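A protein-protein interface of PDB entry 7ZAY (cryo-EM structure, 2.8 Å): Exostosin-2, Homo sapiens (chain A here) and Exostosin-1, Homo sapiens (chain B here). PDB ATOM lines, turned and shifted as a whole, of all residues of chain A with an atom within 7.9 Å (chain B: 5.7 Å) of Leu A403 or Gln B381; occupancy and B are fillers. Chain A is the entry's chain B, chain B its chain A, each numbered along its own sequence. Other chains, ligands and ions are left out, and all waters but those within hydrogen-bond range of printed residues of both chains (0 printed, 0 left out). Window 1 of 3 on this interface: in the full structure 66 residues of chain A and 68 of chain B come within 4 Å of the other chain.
Among the printed residues, pairs that only touch across the chains: Leu A401 with Gln B381 (3.2 Å), Leu A405 with Leu B226 (3.3 Å), Phe A402 with Ala B378 (3.5 Å), Phe A402 with Gln B382 (3.5 Å), Leu A401 with Leu B377 (3.6 Å), Leu A403 with Gln B384 (3.6 Å), Leu A403 with Leu B226 (3.8 Å), Pro A400 with Leu B377 (3.8 Å) and Tyr A560 with Leu B377 (3.95 Å).
The backbone NH of Leu B226 sits at hydrogen-bond distance from the side-chain amide oxygen of Gln B384 (3.2 Å).
The side-chain amide nitrogen of Asn A399 lies within hydrogen-bond range of the backbone carbonyl oxygen of Leu A401, at 2.5 Å.
NE2 of His A558 sits at hydrogen-bond distance from O of Asn B229 (3.5 Å).
The side-chain amide nitrogen of Gln B381 is in hydrogen-bond range of the backbone carbonyl oxygen of Pro A400 (2.5 Å).
The side-chain amide oxygen (OE1) of Gln B381 is in hydrogen-bond range of the backbone NH (N) of Phe A402.
OE1 of Gln B381 lies within hydrogen-bond range of N of Leu A403, 2.7 Å away.
Hydrophobic or aromatic side chains of chain A within 4 Å of the printed part of chain B: Leu A401, Phe A402, Leu A403, Leu A405, His A558 and Tyr A560.
Of the 13 printed residues of chain B, 7 touch a printed residue of chain A.
Hydrophobic or aromatic side chains of chain B that line the printed part of chain A: Leu B226 and Leu B377.
Among the printed residues, 13 pairs touch across the chains.
Among the printed residues, no Asp or Glu carboxylate lies within 4 Å of a Lys or Arg side-chain nitrogen of the other chain.
Printed residues of chain B within 4 Å of Phe A402: Ala B378 (3.5 Å), Gln B381 (2.7 Å) and Gln B382 (3.5 Å).
Leu A403 touches just these residues of chain B: Leu B226, Gln B381 and Gln B384.
Asp A518 touches none of the printed residues of chain B.
Of the printed residues of chain B, Tyr A560 touches Leu B377 (3.95 Å).
Printed residues of chain A within 4 Å of Leu B377: Pro A400, Leu A401 and Tyr A560.
Gln B381 touches four residues of chain A.
Printed residues of chain A within 4 Å of Gln B382: Phe A402.
Of the printed residues of chain A, Gln B384 touches Leu A403.
Leu B386 touches none of the printed residues of chain A.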
ATOM      1  N   ASN A 399      -3.367   3.174  -7.057  1.00  0.00           N
ATOM      2  CA  ASN A 399      -4.218   3.100  -5.874  1.00  0.00           C
ATOM      3  C   ASN A 399      -4.004   1.778  -5.150  1.00  0.00           C
ATOM      4  O   ASN A 399      -4.174   0.715  -5.761  1.00  0.00           O
ATOM      5  CB  ASN A 399      -5.680   3.257  -6.277  1.00  0.00           C
ATOM      6  CG  ASN A 399      -6.623   3.187  -5.095  1.00  0.00           C
ATOM      7  OD1 ASN A 399      -6.252   3.511  -3.968  1.00  0.00           O
ATOM      8  ND2 ASN A 399      -7.857   2.766  -5.348  1.00  0.00           N
ATOM      9  N   PRO A 400      -3.623   1.788  -3.869  1.00  0.00           N
ATOM     10  CA  PRO A 400      -3.429   0.515  -3.155  1.00  0.00           C
ATOM     11  C   PRO A 400      -4.690  -0.324  -3.063  1.00  0.00           C
ATOM     12  O   PRO A 400      -4.607  -1.558  -3.097  1.00  0.00           O
ATOM     13  CB  PRO A 400      -2.948   0.963  -1.768  1.00  0.00           C
ATOM     14  CG  PRO A 400      -2.405   2.337  -1.976  1.00  0.00           C
ATOM     15  CD  PRO A 400      -3.260   2.947  -3.039  1.00  0.00           C
ATOM     16  N   LEU A 401      -5.858   0.308  -2.945  1.00  0.00           N
ATOM     17  CA  LEU A 401      -7.134  -0.402  -2.911  1.00  0.00           C
ATOM     18  C   LEU A 401      -7.798  -0.249  -4.276  1.00  0.00           C
ATOM     19  O   LEU A 401      -8.670   0.594  -4.488  1.00  0.00           O
ATOM     20  CB  LEU A 401      -8.015   0.133  -1.785  1.00  0.00           C
ATOM     21  CG  LEU A 401      -7.378   0.242  -0.399  1.00  0.00           C
ATOM     22  CD1 LEU A 401      -8.167   1.191   0.483  1.00  0.00           C
ATOM     23  CD2 LEU A 401      -7.297  -1.125   0.250  1.00  0.00           C
ATOM     24  N   PHE A 402      -7.372  -1.090  -5.218  1.00  0.00           N
ATOM     25  CA  PHE A 402      -7.846  -0.992  -6.592  1.00  0.00           C
ATOM     26  C   PHE A 402      -8.958  -1.978  -6.920  1.00  0.00           C
ATOM     27  O   PHE A 402      -9.633  -1.805  -7.939  1.00  0.00           O
ATOM     28  CB  PHE A 402      -6.683  -1.183  -7.577  1.00  0.00           C
ATOM     29  CG  PHE A 402      -5.893  -2.442  -7.361  1.00  0.00           C
ATOM     30  CD1 PHE A 402      -4.801  -2.452  -6.510  1.00  0.00           C
ATOM     31  CD2 PHE A 402      -6.226  -3.609  -8.026  1.00  0.00           C
ATOM     32  CE1 PHE A 402      -4.066  -3.603  -6.314  1.00  0.00           C
ATOM     33  CE2 PHE A 402      -5.494  -4.763  -7.835  1.00  0.00           C
ATOM     34  CZ  PHE A 402      -4.412  -4.760  -6.978  1.00  0.00           C
ATOM     35  N   LEU A 403      -9.161  -2.995  -6.095  1.00  0.00           N
ATOM     36  CA  LEU A 403     -10.242  -3.945  -6.324  1.00  0.00           C
ATOM     37  C   LEU A 403     -11.583  -3.264  -6.086  1.00  0.00           C
ATOM     38  O   LEU A 403     -11.825  -2.761  -4.980  1.00  0.00           O
ATOM     39  CB  LEU A 403     -10.082  -5.151  -5.406  1.00  0.00           C
ATOM     40  CG  LEU A 403     -11.120  -6.268  -5.500  1.00  0.00           C
ATOM     41  CD1 LEU A 403     -11.204  -6.808  -6.917  1.00  0.00           C
ATOM     42  CD2 LEU A 403     -10.765  -7.376  -4.528  1.00  0.00           C
ATOM     43  N   PRO A 404     -12.477  -3.220  -7.074  1.00  0.00           N
ATOM     44  CA  PRO A 404     -13.758  -2.503  -6.925  1.00  0.00           C
ATOM     45  C   PRO A 404     -14.809  -3.308  -6.164  1.00  0.00           C
ATOM     46  O   PRO A 404     -15.914  -3.561  -6.651  1.00  0.00           O
ATOM     47  CB  PRO A 404     -14.155  -2.246  -8.385  1.00  0.00           C
ATOM     48  CG  PRO A 404     -13.572  -3.391  -9.127  1.00  0.00           C
ATOM     49  CD  PRO A 404     -12.271  -3.709  -8.448  1.00  0.00           C
ATOM     50  N   LEU A 405     -14.465  -3.719  -4.947  1.00  0.00           N
ATOM     51  CA  LEU A 405     -15.411  -4.438  -4.109  1.00  0.00           C
ATOM     52  C   LEU A 405     -16.478  -3.497  -3.554  1.00  0.00           C
ATOM     53  O   LEU A 405     -16.335  -2.272  -3.560  1.00  0.00           O
ATOM     54  CB  LEU A 405     -14.692  -5.128  -2.950  1.00  0.00           C
ATOM     55  CG  LEU A 405     -14.055  -6.491  -3.215  1.00  0.00           C
ATOM     56  CD1 LEU A 405     -13.292  -6.958  -1.988  1.00  0.00           C
ATOM     57  CD2 LEU A 405     -15.113  -7.507  -3.612  1.00  0.00           C
ATOM     58  N   ILE A 406     -17.563  -4.096  -3.072  1.00  0.00           N
ATOM     59  CA  ILE A 406     -18.561  -3.396  -2.265  1.00  0.00           C
ATOM     60  C   ILE A 406     -18.847  -4.253  -1.037  1.00  0.00           C
ATOM     61  O   ILE A 406     -19.413  -5.347  -1.167  1.00  0.00           O
ATOM     62  CB  ILE A 406     -19.842  -3.114  -3.065  1.00  0.00           C
ATOM     63  CG1 ILE A 406     -19.583  -2.048  -4.132  1.00  0.00           C
ATOM     64  CG2 ILE A 406     -20.961  -2.670  -2.135  1.00  0.00           C
ATOM     65  CD1 ILE A 406     -20.840  -1.505  -4.776  1.00  0.00           C
ATOM     66  N   PRO A 517     -15.102   2.156  -0.774  1.00  0.00           N
ATOM     67  CA  PRO A 517     -14.346   1.738   0.414  1.00  0.00           C
ATOM     68  C   PRO A 517     -12.907   2.227   0.437  1.00  0.00           C
ATOM     69  O   PRO A 517     -12.194   1.943   1.404  1.00  0.00           O
ATOM     70  CB  PRO A 517     -14.406   0.206   0.339  1.00  0.00           C
ATOM     71  CG  PRO A 517     -14.558  -0.085  -1.111  1.00  0.00           C
ATOM     72  CD  PRO A 517     -15.405   1.023  -1.666  1.00  0.00           C
ATOM     73  N   ASP A 518     -12.457   2.948  -0.590  1.00  0.00           N
ATOM     74  CA  ASP A 518     -11.098   3.474  -0.643  1.00  0.00           C
ATOM     75  C   ASP A 518     -11.060   4.993  -0.730  1.00  0.00           C
ATOM     76  O   ASP A 518     -10.004   5.558  -1.040  1.00  0.00           O
ATOM     77  CB  ASP A 518     -10.342   2.870  -1.830  1.00  0.00           C
ATOM     78  CG  ASP A 518     -10.796   3.434  -3.163  1.00  0.00           C
ATOM     79  OD1 ASP A 518     -12.006   3.693  -3.323  1.00  0.00           O
ATOM     80  OD2 ASP A 518      -9.939   3.619  -4.052  1.00  0.00           O
ATOM     81  N   HIS A 558     -11.396   4.453   5.085  1.00  0.00           N
ATOM     82  CA  HIS A 558     -10.889   3.092   5.170  1.00  0.00           C
ATOM     83  C   HIS A 558      -9.874   2.977   6.301  1.00  0.00           C
ATOM     84  O   HIS A 558      -9.053   3.873   6.512  1.00  0.00           O
ATOM     85  CB  HIS A 558     -10.252   2.684   3.842  1.00  0.00           C
ATOM     86  CG  HIS A 558     -10.202   1.205   3.625  1.00  0.00           C
ATOM     87  ND1 HIS A 558     -11.055   0.551   2.762  1.00  0.00           N
ATOM     88  CD2 HIS A 558      -9.405   0.251   4.159  1.00  0.00           C
ATOM     89  CE1 HIS A 558     -10.783  -0.741   2.773  1.00  0.00           C
ATOM     90  NE2 HIS A 558      -9.786  -0.950   3.613  1.00  0.00           N
ATOM     91  N   TYR A 560      -7.315   1.366   6.382  1.00  0.00           N
ATOM     92  CA  TYR A 560      -5.966   1.407   5.829  1.00  0.00           C
ATOM     93  C   TYR A 560      -5.358   2.800   5.912  1.00  0.00           C
ATOM     94  O   TYR A 560      -4.128   2.931   5.920  1.00  0.00           O
ATOM     95  CB  TYR A 560      -5.992   0.930   4.375  1.00  0.00           C
ATOM     96  CG  TYR A 560      -4.631   0.723   3.754  1.00  0.00           C
ATOM     97  CD1 TYR A 560      -3.869  -0.398   4.060  1.00  0.00           C
ATOM     98  CD2 TYR A 560      -4.111   1.641   2.852  1.00  0.00           C
ATOM     99  CE1 TYR A 560      -2.626  -0.592   3.492  1.00  0.00           C
ATOM    100  CE2 TYR A 560      -2.870   1.454   2.278  1.00  0.00           C
ATOM    101  CZ  TYR A 560      -2.131   0.336   2.600  1.00  0.00           C
ATOM    102  OH  TYR A 560      -0.894   0.148   2.029  1.00  0.00           O
ATOM    103  N   LYS A 598      -7.814  10.110  -6.319  1.00  0.00           N
ATOM    104  CA  LYS A 598      -9.257  10.225  -6.447  1.00  0.00           C
ATOM    105  C   LYS A 598      -9.736  11.362  -5.559  1.00  0.00           C
ATOM    106  O   LYS A 598      -8.990  11.889  -4.729  1.00  0.00           O
ATOM    107  CB  LYS A 598      -9.960   8.908  -6.089  1.00  0.00           C
ATOM    108  CG  LYS A 598      -9.610   7.757  -7.021  1.00  0.00           C
ATOM    109  CD  LYS A 598     -10.216   6.445  -6.556  1.00  0.00           C
ATOM    110  CE  LYS A 598      -9.878   5.317  -7.517  1.00  0.00           C
ATOM    111  NZ  LYS A 598     -10.511   4.033  -7.114  1.00  0.00           N
ATOM    112  N   LEU B 226     -13.528 -13.033  -1.517  1.00  0.00           N
ATOM    113  CA  LEU B 226     -12.852 -12.053  -0.676  1.00  0.00           C
ATOM    114  C   LEU B 226     -13.794 -10.903  -0.367  1.00  0.00           C
ATOM    115  O   LEU B 226     -14.090 -10.073  -1.233  1.00  0.00           O
ATOM    116  CB  LEU B 226     -11.588 -11.529  -1.347  1.00  0.00           C
ATOM    117  CG  LEU B 226     -10.902 -10.417  -0.548  1.00  0.00           C
ATOM    118  CD1 LEU B 226     -10.052 -11.002   0.570  1.00  0.00           C
ATOM    119  CD2 LEU B 226     -10.070  -9.514  -1.446  1.00  0.00           C
ATOM    120  N   ASN B 229     -12.083  -6.461   3.451  1.00  0.00           N
ATOM    121  CA  ASN B 229     -10.670  -6.179   3.184  1.00  0.00           C
ATOM    122  C   ASN B 229     -10.042  -5.534   4.417  1.00  0.00           C
ATOM    123  O   ASN B 229      -9.848  -4.319   4.501  1.00  0.00           O
ATOM    124  CB  ASN B 229     -10.521  -5.286   1.957  1.00  0.00           C
ATOM    125  CG  ASN B 229      -9.339  -5.676   1.090  1.00  0.00           C
ATOM    126  OD1 ASN B 229      -8.438  -6.390   1.532  1.00  0.00           O
ATOM    127  ND2 ASN B 229      -9.333  -5.202  -0.151  1.00  0.00           N
ATOM    128  N   ILE B 376       1.083  -7.709   0.221  1.00  0.00           N
ATOM    129  CA  ILE B 376       0.054  -8.721   0.444  1.00  0.00           C
ATOM    130  C   ILE B 376      -1.308  -8.204   0.000  1.00  0.00           C
ATOM    131  O   ILE B 376      -2.093  -8.930  -0.620  1.00  0.00           O
ATOM    132  CB  ILE B 376       0.038  -9.155   1.921  1.00  0.00           C
ATOM    133  CG1 ILE B 376       1.326  -9.893   2.280  1.00  0.00           C
ATOM    134  CG2 ILE B 376      -1.161 -10.040   2.208  1.00  0.00           C
ATOM    135  CD1 ILE B 376       1.400 -10.325   3.725  1.00  0.00           C
ATOM    136  N   LEU B 377      -1.609  -6.943   0.309  1.00  0.00           N
ATOM    137  CA  LEU B 377      -2.880  -6.356  -0.105  1.00  0.00           C
ATOM    138  C   LEU B 377      -2.995  -6.306  -1.624  1.00  0.00           C
ATOM    139  O   LEU B 377      -4.043  -6.648  -2.193  1.00  0.00           O
ATOM    140  CB  LEU B 377      -3.013  -4.957   0.495  1.00  0.00           C
ATOM    141  CG  LEU B 377      -4.353  -4.231   0.389  1.00  0.00           C
ATOM    142  CD1 LEU B 377      -5.328  -4.739   1.439  1.00  0.00           C
ATOM    143  CD2 LEU B 377      -4.133  -2.736   0.530  1.00  0.00           C
ATOM    144  N   ALA B 378      -1.922  -5.880  -2.294  1.00  0.00           N
ATOM    145  CA  ALA B 378      -1.937  -5.821  -3.752  1.00  0.00           C
ATOM    146  C   ALA B 378      -2.090  -7.211  -4.355  1.00  0.00           C
ATOM    147  O   ALA B 378      -2.837  -7.397  -5.322  1.00  0.00           O
ATOM    148  CB  ALA B 378      -0.665  -5.147  -4.264  1.00  0.00           C
ATOM    149  N   LEU B 379      -1.398  -8.204  -3.788  1.00  0.00           N
ATOM    150  CA  LEU B 379      -1.523  -9.576  -4.269  1.00  0.00           C
ATOM    151  C   LEU B 379      -2.942 -10.097  -4.088  1.00  0.00           C
ATOM    152  O   LEU B 379      -3.478 -10.773  -4.969  1.00  0.00           O
ATOM    153  CB  LEU B 379      -0.528 -10.481  -3.540  1.00  0.00           C
ATOM    154  CG  LEU B 379       0.958 -10.322  -3.865  1.00  0.00           C
ATOM    155  CD1 LEU B 379       1.806 -10.870  -2.731  1.00  0.00           C
ATOM    156  CD2 LEU B 379       1.297 -11.024  -5.163  1.00  0.00           C
ATOM    157  N   ARG B 380      -3.565  -9.786  -2.950  1.00  0.00           N
ATOM    158  CA  ARG B 380      -4.937 -10.215  -2.693  1.00  0.00           C
ATOM    159  C   ARG B 380      -5.898  -9.634  -3.726  1.00  0.00           C
ATOM    160  O   ARG B 380      -6.683 -10.362  -4.356  1.00  0.00           O
ATOM    161  CB  ARG B 380      -5.337  -9.777  -1.283  1.00  0.00           C
ATOM    162  CG  ARG B 380      -6.576 -10.432  -0.717  1.00  0.00           C
ATOM    163  CD  ARG B 380      -6.265 -11.807  -0.164  1.00  0.00           C
ATOM    164  NE  ARG B 380      -5.094 -11.811   0.704  1.00  0.00           N
ATOM    165  CZ  ARG B 380      -5.133 -11.614   2.014  1.00  0.00           C
ATOM    166  NH1 ARG B 380      -6.268 -11.354   2.640  1.00  0.00           N
ATOM    167  NH2 ARG B 380      -4.004 -11.676   2.713  1.00  0.00           N
ATOM    168  N   GLN B 381      -5.842  -8.313  -3.916  1.00  0.00           N
ATOM    169  CA  GLN B 381      -6.756  -7.674  -4.856  1.00  0.00           C
ATOM    170  C   GLN B 381      -6.497  -8.136  -6.285  1.00  0.00           C
ATOM    171  O   GLN B 381      -7.439  -8.326  -7.063  1.00  0.00           O
ATOM    172  CB  GLN B 381      -6.647  -6.156  -4.748  1.00  0.00           C
ATOM    173  CG  GLN B 381      -6.928  -5.616  -3.359  1.00  0.00           C
ATOM    174  CD  GLN B 381      -6.863  -4.107  -3.305  1.00  0.00           C
ATOM    175  OE1 GLN B 381      -7.656  -3.418  -3.943  1.00  0.00           O
ATOM    176  NE2 GLN B 381      -5.908  -3.584  -2.546  1.00  0.00           N
ATOM    177  N   GLN B 382      -5.226  -8.332  -6.651  1.00  0.00           N
ATOM    178  CA  GLN B 382      -4.913  -8.796  -7.997  1.00  0.00           C
ATOM    179  C   GLN B 382      -5.374 -10.232  -8.206  1.00  0.00           C
ATOM    180  O   GLN B 382      -5.818 -10.593  -9.301  1.00  0.00           O
ATOM    181  CB  GLN B 382      -3.412  -8.663  -8.260  1.00  0.00           C
ATOM    182  CG  GLN B 382      -2.997  -8.925  -9.701  1.00  0.00           C
ATOM    183  CD  GLN B 382      -3.440  -7.834 -10.658  1.00  0.00           C
ATOM    184  OE1 GLN B 382      -4.031  -6.832 -10.255  1.00  0.00           O
ATOM    185  NE2 GLN B 382      -3.154  -8.026 -11.940  1.00  0.00           N
ATOM    186  N   THR B 383      -5.251 -11.070  -7.175  1.00  0.00           N
ATOM    187  CA  THR B 383      -5.797 -12.420  -7.226  1.00  0.00           C
ATOM    188  C   THR B 383      -7.288 -12.391  -7.531  1.00  0.00           C
ATOM    189  O   THR B 383      -7.767 -13.104  -8.424  1.00  0.00           O
ATOM    190  CB  THR B 383      -5.528 -13.129  -5.895  1.00  0.00           C
ATOM    191  OG1 THR B 383      -4.132 -13.430  -5.783  1.00  0.00           O
ATOM    192  CG2 THR B 383      -6.335 -14.405  -5.778  1.00  0.00           C
ATOM    193  N   GLN B 384      -8.036 -11.562  -6.802  1.00  0.00           N
ATOM    194  CA  GLN B 384      -9.472 -11.468  -7.061  1.00  0.00           C
ATOM    195  C   GLN B 384      -9.759 -10.949  -8.467  1.00  0.00           C
ATOM    196  O   GLN B 384     -10.659 -11.455  -9.154  1.00  0.00           O
ATOM    197  CB  GLN B 384     -10.139 -10.587  -6.010  1.00  0.00           C
ATOM    198  CG  GLN B 384     -10.163 -11.209  -4.634  1.00  0.00           C
ATOM    199  CD  GLN B 384     -10.963 -12.496  -4.602  1.00  0.00           C
ATOM    200  OE1 GLN B 384     -12.161 -12.481  -4.332  1.00  0.00           O
ATOM    201  NE2 GLN B 384     -10.306 -13.616  -4.875  1.00  0.00           N
ATOM    202  N   PHE B 385      -9.009  -9.937  -8.907  1.00  0.00           N
ATOM    203  CA  PHE B 385      -9.207  -9.398 -10.248  1.00  0.00           C
ATOM    204  C   PHE B 385      -8.983 -10.468 -11.306  1.00  0.00           C
ATOM    205  O   PHE B 385      -9.797 -10.631 -12.222  1.00  0.00           O
ATOM    206  CB  PHE B 385      -8.272  -8.213 -10.485  1.00  0.00           C
ATOM    207  CG  PHE B 385      -7.892  -8.026 -11.926  1.00  0.00           C
ATOM    208  CD1 PHE B 385      -8.794  -7.495 -12.832  1.00  0.00           C
ATOM    209  CD2 PHE B 385      -6.636  -8.396 -12.377  1.00  0.00           C
ATOM    210  CE1 PHE B 385      -8.448  -7.334 -14.157  1.00  0.00           C
ATOM    211  CE2 PHE B 385      -6.287  -8.237 -13.700  1.00  0.00           C
ATOM    212  CZ  PHE B 385      -7.193  -7.710 -14.591  1.00  0.00           C
ATOM    213  N   LEU B 386      -7.880 -11.211 -11.195  1.00  0.00           N
ATOM    214  CA  LEU B 386      -7.573 -12.228 -12.193  1.00  0.00           C
ATOM    215  C   LEU B 386      -8.618 -13.333 -12.188  1.00  0.00           C
ATOM    216  O   LEU B 386      -9.067 -13.774 -13.253  1.00  0.00           O
ATOM    217  CB  LEU B 386      -6.180 -12.806 -11.950  1.00  0.00           C
ATOM    218  CG  LEU B 386      -5.004 -12.033 -12.544  1.00  0.00           C
ATOM    219  CD1 LEU B 386      -3.752 -12.881 -12.499  1.00  0.00           C
ATOM    220  CD2 LEU B 386      -5.307 -11.603 -13.966  1.00  0.00           C
